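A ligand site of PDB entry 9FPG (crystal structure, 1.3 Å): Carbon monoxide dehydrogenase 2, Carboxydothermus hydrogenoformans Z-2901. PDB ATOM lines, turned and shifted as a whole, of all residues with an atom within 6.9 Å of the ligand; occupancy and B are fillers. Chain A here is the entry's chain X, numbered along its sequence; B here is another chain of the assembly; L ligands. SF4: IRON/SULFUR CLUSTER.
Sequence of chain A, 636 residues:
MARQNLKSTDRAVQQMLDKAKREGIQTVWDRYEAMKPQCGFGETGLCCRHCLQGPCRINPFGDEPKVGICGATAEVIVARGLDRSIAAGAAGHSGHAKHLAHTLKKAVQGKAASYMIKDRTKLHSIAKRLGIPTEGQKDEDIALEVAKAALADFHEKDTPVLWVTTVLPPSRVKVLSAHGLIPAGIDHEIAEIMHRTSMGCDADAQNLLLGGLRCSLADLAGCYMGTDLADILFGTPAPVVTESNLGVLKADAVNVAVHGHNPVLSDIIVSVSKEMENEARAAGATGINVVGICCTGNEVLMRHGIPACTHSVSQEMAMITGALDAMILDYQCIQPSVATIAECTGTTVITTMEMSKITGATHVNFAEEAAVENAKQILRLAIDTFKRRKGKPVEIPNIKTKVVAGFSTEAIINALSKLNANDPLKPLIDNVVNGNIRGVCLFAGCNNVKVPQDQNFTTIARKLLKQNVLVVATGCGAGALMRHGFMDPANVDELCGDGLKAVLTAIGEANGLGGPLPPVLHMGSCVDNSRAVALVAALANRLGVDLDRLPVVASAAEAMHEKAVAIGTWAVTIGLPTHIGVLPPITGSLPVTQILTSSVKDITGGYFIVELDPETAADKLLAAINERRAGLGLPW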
ATOM      1  N   CYS A  47     -18.252  16.583   5.893  1.00  0.00           N
ATOM      2  CA  CYS A  47     -18.749  15.431   6.647  1.00  0.00           C
ATOM      3  C   CYS A  47     -17.547  14.768   7.314  1.00  0.00           C
ATOM      4  O   CYS A  47     -16.472  14.645   6.704  1.00  0.00           O
ATOM      5  CB  CYS A  47     -19.476  14.421   5.761  1.00  0.00           C
ATOM      6  SG  CYS A  47     -20.072  13.002   6.720  1.00  0.00           S
ATOM      7  N   CYS A  48     -17.715  14.349   8.559  1.00  0.00           N
ATOM      8  CA  CYS A  48     -16.661  13.649   9.283  1.00  0.00           C
ATOM      9  C   CYS A  48     -17.281  12.480  10.033  1.00  0.00           C
ATOM     10  O   CYS A  48     -18.297  12.641  10.718  1.00  0.00           O
ATOM     11  CB  CYS A  48     -15.965  14.576  10.266  1.00  0.00           C
ATOM     12  SG  CYS A  48     -14.675  13.786  11.253  1.00  0.00           S
ATOM     13  N   ARG A  49     -16.664  11.307   9.880  1.00  0.00           N
ATOM     14  CA  ARG A  49     -16.996  10.105  10.632  1.00  0.00           C
ATOM     15  C   ARG A  49     -15.774   9.548  11.366  1.00  0.00           C
ATOM     16  O   ARG A  49     -15.645   8.339  11.523  1.00  0.00           O
ATOM     17  CB  ARG A  49     -17.613   9.061   9.702  1.00  0.00           C
ATOM     18  CG  ARG A  49     -18.893   9.540   9.041  1.00  0.00           C
ATOM     19  CD  ARG A  49     -19.273   8.634   7.880  1.00  0.00           C
ATOM     20  NE  ARG A  49     -19.487   7.285   8.353  1.00  0.00           N
ATOM     21  CZ  ARG A  49     -19.411   6.179   7.622  1.00  0.00           C
ATOM     22  NH1 ARG A  49     -19.181   6.226   6.327  1.00  0.00           N
ATOM     23  NH2 ARG A  49     -19.568   4.999   8.221  1.00  0.00           N
ATOM     24  N   HIS A  50     -14.877  10.418  11.816  1.00  0.00           N
ATOM     25  CA  HIS A  50     -13.641   9.951  12.436  1.00  0.00           C
ATOM     26  C   HIS A  50     -13.810   9.533  13.888  1.00  0.00           C
ATOM     27  O   HIS A  50     -12.822   9.087  14.497  1.00  0.00           O
ATOM     28  CB  HIS A  50     -12.522  10.981  12.304  1.00  0.00           C
ATOM     29  CG  HIS A  50     -12.050  11.183  10.894  1.00  0.00           C
ATOM     30  ND1 HIS A  50     -10.859  11.799  10.589  1.00  0.00           N
ATOM     31  CD2 HIS A  50     -12.623  10.853   9.707  1.00  0.00           C
ATOM     32  CE1 HIS A  50     -10.715  11.835   9.266  1.00  0.00           C
ATOM     33  NE2 HIS A  50     -11.764  11.279   8.708  1.00  0.00           N
ATOM     34  N   CYS A  51     -15.011   9.621  14.458  1.00  0.00           N
ATOM     35  CA  CYS A  51     -15.255   9.012  15.766  1.00  0.00           C
ATOM     36  C   CYS A  51     -16.726   8.663  15.907  1.00  0.00           C
ATOM     37  O   CYS A  51     -17.553   9.045  15.087  1.00  0.00           O
ATOM     38  CB  CYS A  51     -14.784   9.908  16.931  1.00  0.00           C
ATOM     39  SG  CYS A  51     -15.923  11.262  17.445  1.00  0.00           S
ATOM     40  N   LEU A  52     -17.040   7.938  16.984  1.00  0.00           N
ATOM     41  CA  LEU A  52     -18.401   7.444  17.194  1.00  0.00           C
ATOM     42  C   LEU A  52     -19.356   8.475  17.792  1.00  0.00           C
ATOM     43  O   LEU A  52     -20.497   8.138  18.072  1.00  0.00           O
ATOM     44  CB  LEU A  52     -18.385   6.174  18.054  1.00  0.00           C
ATOM     45  CG  LEU A  52     -17.563   5.021  17.487  1.00  0.00           C
ATOM     46  CD1 LEU A  52     -17.653   3.804  18.415  1.00  0.00           C
ATOM     47  CD2 LEU A  52     -18.034   4.641  16.090  1.00  0.00           C
ATOM     48  N   GLN A  53     -18.918   9.733  17.974  1.00  0.00           N
ATOM     49  CA  GLN A  53     -19.849  10.810  18.221  1.00  0.00           C
ATOM     50  C   GLN A  53     -20.512  11.291  16.944  1.00  0.00           C
ATOM     51  O   GLN A  53     -21.572  11.928  17.009  1.00  0.00           O
ATOM     52  CB  GLN A  53     -19.145  11.967  18.941  1.00  0.00           C
ATOM     53  CG  GLN A  53     -18.758  11.568  20.357  1.00  0.00           C
ATOM     54  CD  GLN A  53     -18.049  12.647  21.151  1.00  0.00           C
ATOM     55  OE1 GLN A  53     -18.166  12.681  22.374  1.00  0.00           O
ATOM     56  NE2 GLN A  53     -17.294  13.504  20.472  1.00  0.00           N
ATOM     57  N   GLY A  54     -19.920  10.992  15.784  1.00  0.00           N
ATOM     58  CA  GLY A  54     -20.474  11.395  14.524  1.00  0.00           C
ATOM     59  C   GLY A  54     -21.595  10.456  14.118  1.00  0.00           C
ATOM     60  O   GLY A  54     -22.013   9.577  14.871  1.00  0.00           O
ATOM     61  N   PRO A  55     -22.063  10.606  12.890  1.00  0.00           N
ATOM     62  CA  PRO A  55     -21.497  11.479  11.857  1.00  0.00           C
ATOM     63  C   PRO A  55     -21.751  12.948  12.121  1.00  0.00           C
ATOM     64  O   PRO A  55     -22.805  13.350  12.594  1.00  0.00           O
ATOM     65  CB  PRO A  55     -22.210  11.028  10.572  1.00  0.00           C
ATOM     66  CG  PRO A  55     -23.471  10.358  11.036  1.00  0.00           C
ATOM     67  CD  PRO A  55     -23.174   9.779  12.392  1.00  0.00           C
ATOM     68  N   CYS A  56     -20.745  13.759  11.810  1.00  0.00           N
ATOM     69  CA  CYS A  56     -20.839  15.194  11.879  1.00  0.00           C
ATOM     70  C   CYS A  56     -20.883  15.744  10.463  1.00  0.00           C
ATOM     71  O   CYS A  56     -20.257  15.203   9.543  1.00  0.00           O
ATOM     72  CB  CYS A  56     -19.647  15.792  12.624  1.00  0.00           C
ATOM     73  SG  CYS A  56     -19.648  15.443  14.419  1.00  0.00           S
ATOM     74  N   ARG A  57     -21.628  16.817  10.291  1.00  0.00           N
ATOM     75  CA  ARG A  57     -21.686  17.520   9.026  1.00  0.00           C
ATOM     76  C   ARG A  57     -21.716  19.003   9.343  1.00  0.00           C
ATOM     77  O   ARG A  57     -21.995  19.420  10.482  1.00  0.00           O
ATOM     78  CB  ARG A  57     -22.913  17.106   8.230  1.00  0.00           C
ATOM     79  CG  ARG A  57     -24.194  17.627   8.830  1.00  0.00           C
ATOM     80  CD  ARG A  57     -25.411  16.896   8.338  1.00  0.00           C
ATOM     81  NE  ARG A  57     -26.613  17.530   8.884  1.00  0.00           N
ATOM     82  CZ  ARG A  57     -27.014  17.412  10.137  1.00  0.00           C
ATOM     83  NH1 ARG A  57     -26.391  16.600  10.988  1.00  0.00           N
ATOM     84  NH2 ARG A  57     -28.055  18.124  10.553  1.00  0.00           N
ATOM     85  N   VAL A  67     -20.138  23.549  13.027  1.00  0.00           N
ATOM     86  CA  VAL A  67     -18.886  23.041  13.561  1.00  0.00           C
ATOM     87  C   VAL A  67     -19.127  21.614  14.011  1.00  0.00           C
ATOM     88  O   VAL A  67     -20.239  21.228  14.362  1.00  0.00           O
ATOM     89  CB  VAL A  67     -18.387  23.969  14.682  1.00  0.00           C
ATOM     90  CG1 VAL A  67     -19.414  24.063  15.812  1.00  0.00           C
ATOM     91  CG2 VAL A  67     -17.042  23.536  15.205  1.00  0.00           C
ATOM     92  N   GLY A  68     -18.066  20.808  13.963  1.00  0.00           N
ATOM     93  CA  GLY A  68     -18.159  19.440  14.430  1.00  0.00           C
ATOM     94  C   GLY A  68     -18.359  19.366  15.935  1.00  0.00           C
ATOM     95  O   GLY A  68     -18.100  20.308  16.674  1.00  0.00           O
ATOM     96  N   ILE A  69     -18.822  18.206  16.378  1.00  0.00           N
ATOM     97  CA  ILE A  69     -19.172  18.014  17.784  1.00  0.00           C
ATOM     98  C   ILE A  69     -17.965  18.259  18.681  1.00  0.00           C
ATOM     99  O   ILE A  69     -18.090  18.870  19.753  1.00  0.00           O
ATOM    100  CB  ILE A  69     -19.806  16.638  18.004  1.00  0.00           C
ATOM    101  CG1 ILE A  69     -21.223  16.657  17.439  1.00  0.00           C
ATOM    102  CG2 ILE A  69     -19.839  16.282  19.487  1.00  0.00           C
ATOM    103  CD1 ILE A  69     -21.871  15.313  17.415  1.00  0.00           C
ATOM    104  N   CYS A  70     -16.787  17.782  18.284  1.00  0.00           N
ATOM    105  CA  CYS A  70     -15.585  17.980  19.077  1.00  0.00           C
ATOM    106  C   CYS A  70     -14.998  19.371  18.945  1.00  0.00           C
ATOM    107  O   CYS A  70     -13.985  19.681  19.590  1.00  0.00           O
ATOM    108  CB  CYS A  70     -14.522  16.974  18.646  1.00  0.00           C
ATOM    109  SG  CYS A  70     -14.056  17.171  16.892  1.00  0.00           S
ATOM    110  N   GLY A  71     -15.595  20.225  18.093  1.00  0.00           N
ATOM    111  CA  GLY A  71     -15.059  21.534  17.777  1.00  0.00           C
ATOM    112  C   GLY A  71     -14.325  21.633  16.454  1.00  0.00           C
ATOM    113  O   GLY A  71     -13.847  22.717  16.108  1.00  0.00           O
ATOM    114  N   ALA A  72     -14.237  20.549  15.690  1.00  0.00           N
ATOM    115  CA  ALA A  72     -13.515  20.572  14.418  1.00  0.00           C
ATOM    116  C   ALA A  72     -14.213  21.521  13.445  1.00  0.00           C
ATOM    117  O   ALA A  72     -15.398  21.387  13.180  1.00  0.00           O
ATOM    118  CB  ALA A  72     -13.467  19.172  13.837  1.00  0.00           C
ATOM    119  N   THR A  73     -13.435  22.454  12.895  1.00  0.00           N
ATOM    120  CA  THR A  73     -13.980  23.421  11.958  1.00  0.00           C
ATOM    121  C   THR A  73     -14.075  22.810  10.562  1.00  0.00           C
ATOM    122  O   THR A  73     -13.573  21.722  10.284  1.00  0.00           O
ATOM    123  CB  THR A  73     -13.059  24.628  11.874  1.00  0.00           C
ATOM    124  OG1 THR A  73     -11.775  24.164  11.435  1.00  0.00           O
ATOM    125  CG2 THR A  73     -12.927  25.353  13.210  1.00  0.00           C
ATOM    126  N   ILE A  77     -11.987  19.591   9.097  1.00  0.00           N
ATOM    127  CA  ILE A  77     -12.687  18.437   8.542  1.00  0.00           C
ATOM    128  C   ILE A  77     -12.289  18.218   7.081  1.00  0.00           C
ATOM    129  O   ILE A  77     -11.989  17.088   6.666  1.00  0.00           O
ATOM    130  CB  ILE A  77     -14.202  18.626   8.724  1.00  0.00           C
ATOM    131  CG1 ILE A  77     -14.555  18.450  10.209  1.00  0.00           C
ATOM    132  CG2 ILE A  77     -14.984  17.673   7.842  1.00  0.00           C
ATOM    133  CD1 ILE A  77     -15.983  18.810  10.550  1.00  0.00           C
ATOM    134  N   ARG A  80      -8.561  17.041   6.870  1.00  0.00           N
ATOM    135  CA  ARG A  80      -8.354  15.678   7.357  1.00  0.00           C
ATOM    136  C   ARG A  80      -8.867  14.659   6.350  1.00  0.00           C
ATOM    137  O   ARG A  80      -8.209  13.637   6.134  1.00  0.00           O
ATOM    138  CB  ARG A  80      -9.046  15.470   8.708  1.00  0.00           C
ATOM    139  CG  ARG A  80      -8.439  16.285   9.836  1.00  0.00           C
ATOM    140  CD  ARG A  80      -8.915  15.855  11.210  1.00  0.00           C
ATOM    141  NE  ARG A  80     -10.365  15.914  11.343  1.00  0.00           N
ATOM    142  CZ  ARG A  80     -10.978  15.894  12.516  1.00  0.00           C
ATOM    143  NH1 ARG A  80     -10.306  15.863  13.651  1.00  0.00           N
ATOM    144  NH2 ARG A  80     -12.318  15.902  12.554  1.00  0.00           N
ATOM    145  N   THR A 197      -4.918  12.728  11.687  1.00  0.00           N
ATOM    146  CA  THR A 197      -6.278  13.035  11.268  1.00  0.00           C
ATOM    147  C   THR A 197      -7.331  12.360  12.140  1.00  0.00           C
ATOM    148  O   THR A 197      -8.530  12.593  11.946  1.00  0.00           O
ATOM    149  CB  THR A 197      -6.505  12.629   9.810  1.00  0.00           C
ATOM    150  OG1 THR A 197      -6.256  11.233   9.643  1.00  0.00           O
ATOM    151  CG2 THR A 197      -5.632  13.460   8.859  1.00  0.00           C
ATOM    152  N   SER A 198      -6.913  11.513  13.081  1.00  0.00           N
ATOM    153  CA  SER A 198      -7.854  10.903  14.022  1.00  0.00           C
ATOM    154  C   SER A 198      -8.344  11.959  15.022  1.00  0.00           C
ATOM    155  O   SER A 198      -7.798  13.076  15.116  1.00  0.00           O
ATOM    156  CB  SER A 198      -7.233   9.687  14.718  1.00  0.00           C
ATOM    157  OG  SER A 198      -6.264  10.012  15.708  1.00  0.00           O
ATOM    158  N   MET A 199      -9.381  11.610  15.758  1.00  0.00           N
ATOM    159  CA  MET A 199     -10.071  12.590  16.582  1.00  0.00           C
ATOM    160  C   MET A 199      -9.124  13.190  17.616  1.00  0.00           C
ATOM    161  O   MET A 199      -8.335  12.478  18.266  1.00  0.00           O
ATOM    162  CB  MET A 199     -11.277  11.936  17.269  1.00  0.00           C
ATOM    163  CG  MET A 199     -12.132  12.858  18.132  1.00  0.00           C
ATOM    164  SD  MET A 199     -11.502  12.946  19.826  1.00  0.00           S
ATOM    165  CE  MET A 199     -12.765  13.934  20.629  1.00  0.00           C
ATOM    166  N   GLY A 200      -9.202  14.520  17.767  1.00  0.00           N
ATOM    167  CA  GLY A 200      -8.493  15.215  18.830  1.00  0.00           C
ATOM    168  C   GLY A 200      -7.000  15.308  18.620  1.00  0.00           C
ATOM    169  O   GLY A 200      -6.246  15.394  19.594  1.00  0.00           O
ATOM    170  N   VAL B  28     -19.357  20.984  24.080  1.00  0.00           N
ATOM    171  CA  VAL B  28     -19.550  19.768  23.291  1.00  0.00           C
ATOM    172  C   VAL B  28     -21.011  19.336  23.263  1.00  0.00           C
ATOM    173  O   VAL B  28     -21.504  18.838  22.249  1.00  0.00           O
ATOM    174  CB  VAL B  28     -18.615  18.656  23.823  1.00  0.00           C
ATOM    175  CG1 VAL B  28     -19.004  18.243  25.245  1.00  0.00           C
ATOM    176  CG2 VAL B  28     -18.621  17.465  22.889  1.00  0.00           C
ATOM    177  N   MET B  35     -26.205  19.339  16.019  1.00  0.00           N
ATOM    178  CA  MET B  35     -25.988  18.345  14.978  1.00  0.00           C
ATOM    179  C   MET B  35     -27.170  17.419  14.779  1.00  0.00           C
ATOM    180  O   MET B  35     -27.191  16.669  13.792  1.00  0.00           O
ATOM    181  CB  MET B  35     -24.746  17.520  15.341  1.00  0.00           C
ATOM    182  CG  MET B  35     -24.096  16.746  14.216  1.00  0.00           C
ATOM    183  SD  MET B  35     -23.479  17.844  12.890  1.00  0.00           S
ATOM    184  CE  MET B  35     -22.119  18.685  13.694  1.00  0.00           C
ATOM    185  N   GLN B  38     -28.694  13.422  13.390  1.00  0.00           N
ATOM    186  CA  GLN B  38     -27.486  13.045  12.674  1.00  0.00           C
ATOM    187  C   GLN B  38     -27.838  12.147  11.490  1.00  0.00           C
ATOM    188  O   GLN B  38     -28.897  11.517  11.433  1.00  0.00           O
ATOM    189  CB  GLN B  38     -26.523  12.345  13.621  1.00  0.00           C
ATOM    190  CG  GLN B  38     -25.962  13.298  14.659  1.00  0.00           C
ATOM    191  CD  GLN B  38     -25.025  12.626  15.640  1.00  0.00           C
ATOM    192  OE1 GLN B  38     -25.462  12.025  16.601  1.00  0.00           O
ATOM    193  NE2 GLN B  38     -23.732  12.742  15.382  1.00  0.00           N
ATOM    194  N   PRO B 336     -10.666  20.209  19.780  1.00  0.00           N
ATOM    195  CA  PRO B 336     -10.041  21.456  19.329  1.00  0.00           C
ATOM    196  C   PRO B 336     -10.787  22.713  19.748  1.00  0.00           C
ATOM    197  O   PRO B 336     -10.219  23.803  19.665  1.00  0.00           O
ATOM    198  CB  PRO B 336      -9.971  21.285  17.797  1.00  0.00           C
ATOM    199  CG  PRO B 336     -11.056  20.323  17.480  1.00  0.00           C
ATOM    200  CD  PRO B 336     -11.050  19.355  18.644  1.00  0.00           C
ATOM    201  N   MET B 560     -15.799   6.050  21.900  1.00  0.00           N
ATOM    202  CA  MET B 560     -15.814   7.189  20.989  1.00  0.00           C
ATOM    203  C   MET B 560     -14.721   7.119  19.920  1.00  0.00           C
ATOM    204  O   MET B 560     -14.983   7.194  18.715  1.00  0.00           O
ATOM    205  CB  MET B 560     -15.672   8.481  21.805  1.00  0.00           C
ATOM    206  CG  MET B 560     -15.585   9.790  21.011  1.00  0.00           C
ATOM    207  SD  MET B 560     -13.938  10.345  20.558  1.00  0.00           S
ATOM    208  CE  MET B 560     -13.226  10.627  22.147  1.00  0.00           C
HETATM  209 FE1  SF4 L   1     -15.887  12.840  15.811  1.00  0.00          FE
HETATM  210 FE2  SF4 L   1     -17.568  14.691  14.794  1.00  0.00          FE
HETATM  211 FE3  SF4 L   1     -15.359  14.010  13.447  1.00  0.00          FE
HETATM  212 FE4  SF4 L   1     -15.102  15.504  15.671  1.00  0.00          FE
HETATM  213  S1  SF4 L   1     -16.071  16.178  13.763  1.00  0.00           S
HETATM  214  S2  SF4 L   1     -13.839  13.660  15.036  1.00  0.00           S
HETATM  215  S3  SF4 L   1     -16.852  14.618  16.912  1.00  0.00           S
HETATM  216  S4  SF4 L   1     -17.107  12.603  13.940  1.00  0.00           S
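O of Thr 197 sits at hydrogen-bond distance from ND1 of His 50 (2.8 Å). The backbone NH of Cys 48 sits at hydrogen-bond distance from the backbone carbonyl oxygen of Cys 56, at 2.9 Å. The side-chain sulfur of Cys 51 lies close to the backbone NH of Gln 53. The side-chain sulfur (SG) of Cys 48 sits close to the guanidinium group (NH2) of Arg 80 (3.4 Å). The backbone NH (N) of Ala 72 lies close to the side-chain sulfur (SG) of Cys 70 (3.6 Å). The side-chain sulfur of Cys 56 sits close to the backbone NH of Ile 69 (3.5 Å). The side-chain sulfur of Cys 47 lies close to the backbone carbonyl oxygen of Cys 56, at 3.6 Å. SG of Cys 48 lies close to N of His 50, at 3.4 Å.
Residues that only touch the ligand: Gly 68 (3.9 Å), Ile 69 (3.7 Å), Ala 72 (3.97 Å) and Met 199 (3.6 Å). Within 4 Å of the ligand: Cys 48, His 50, Cys 51, Gln 53, Gly 54, Cys 56, Gly 68, Ile 69, Cys 70, Ala 72, Arg 80 and Met 199. The nearest printed residue that does not touch the ligand is Arg 49 (4.1 Å).
An iron atom (FE4) of the ligand is bound by the side-chain sulfur (SG) of Cys 70, 2.3 Å away. S4 of the ligand sits close to N of His 50, 3.8 Å away. The side-chain sulfur (SG) of Cys 56 binds an iron atom (FE2) of the ligand (2.2 Å). NH2 of Arg 80 sits close to S2 of the ligand (3.7 Å). An iron atom (FE1) of the ligand is bound by the side-chain sulfur (SG) of Cys 51 (2.3 Å). The backbone NH (N) of Cys 51 sits close to a sulfur (S4) of the ligand. N of Gly 54 sits close to S4 of the ligand, at 3.7 Å. The side-chain amide nitrogen (NE2) of Gln 53 sits close to a sulfur (S3) of the ligand (3.8 Å). An iron atom (FE3) of the ligand is bound by the side-chain sulfur (SG) of Cys 48. A sulfur (S3) of the ligand sits close to the backbone NH (N) of Cys 70, at 3.4 Å.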
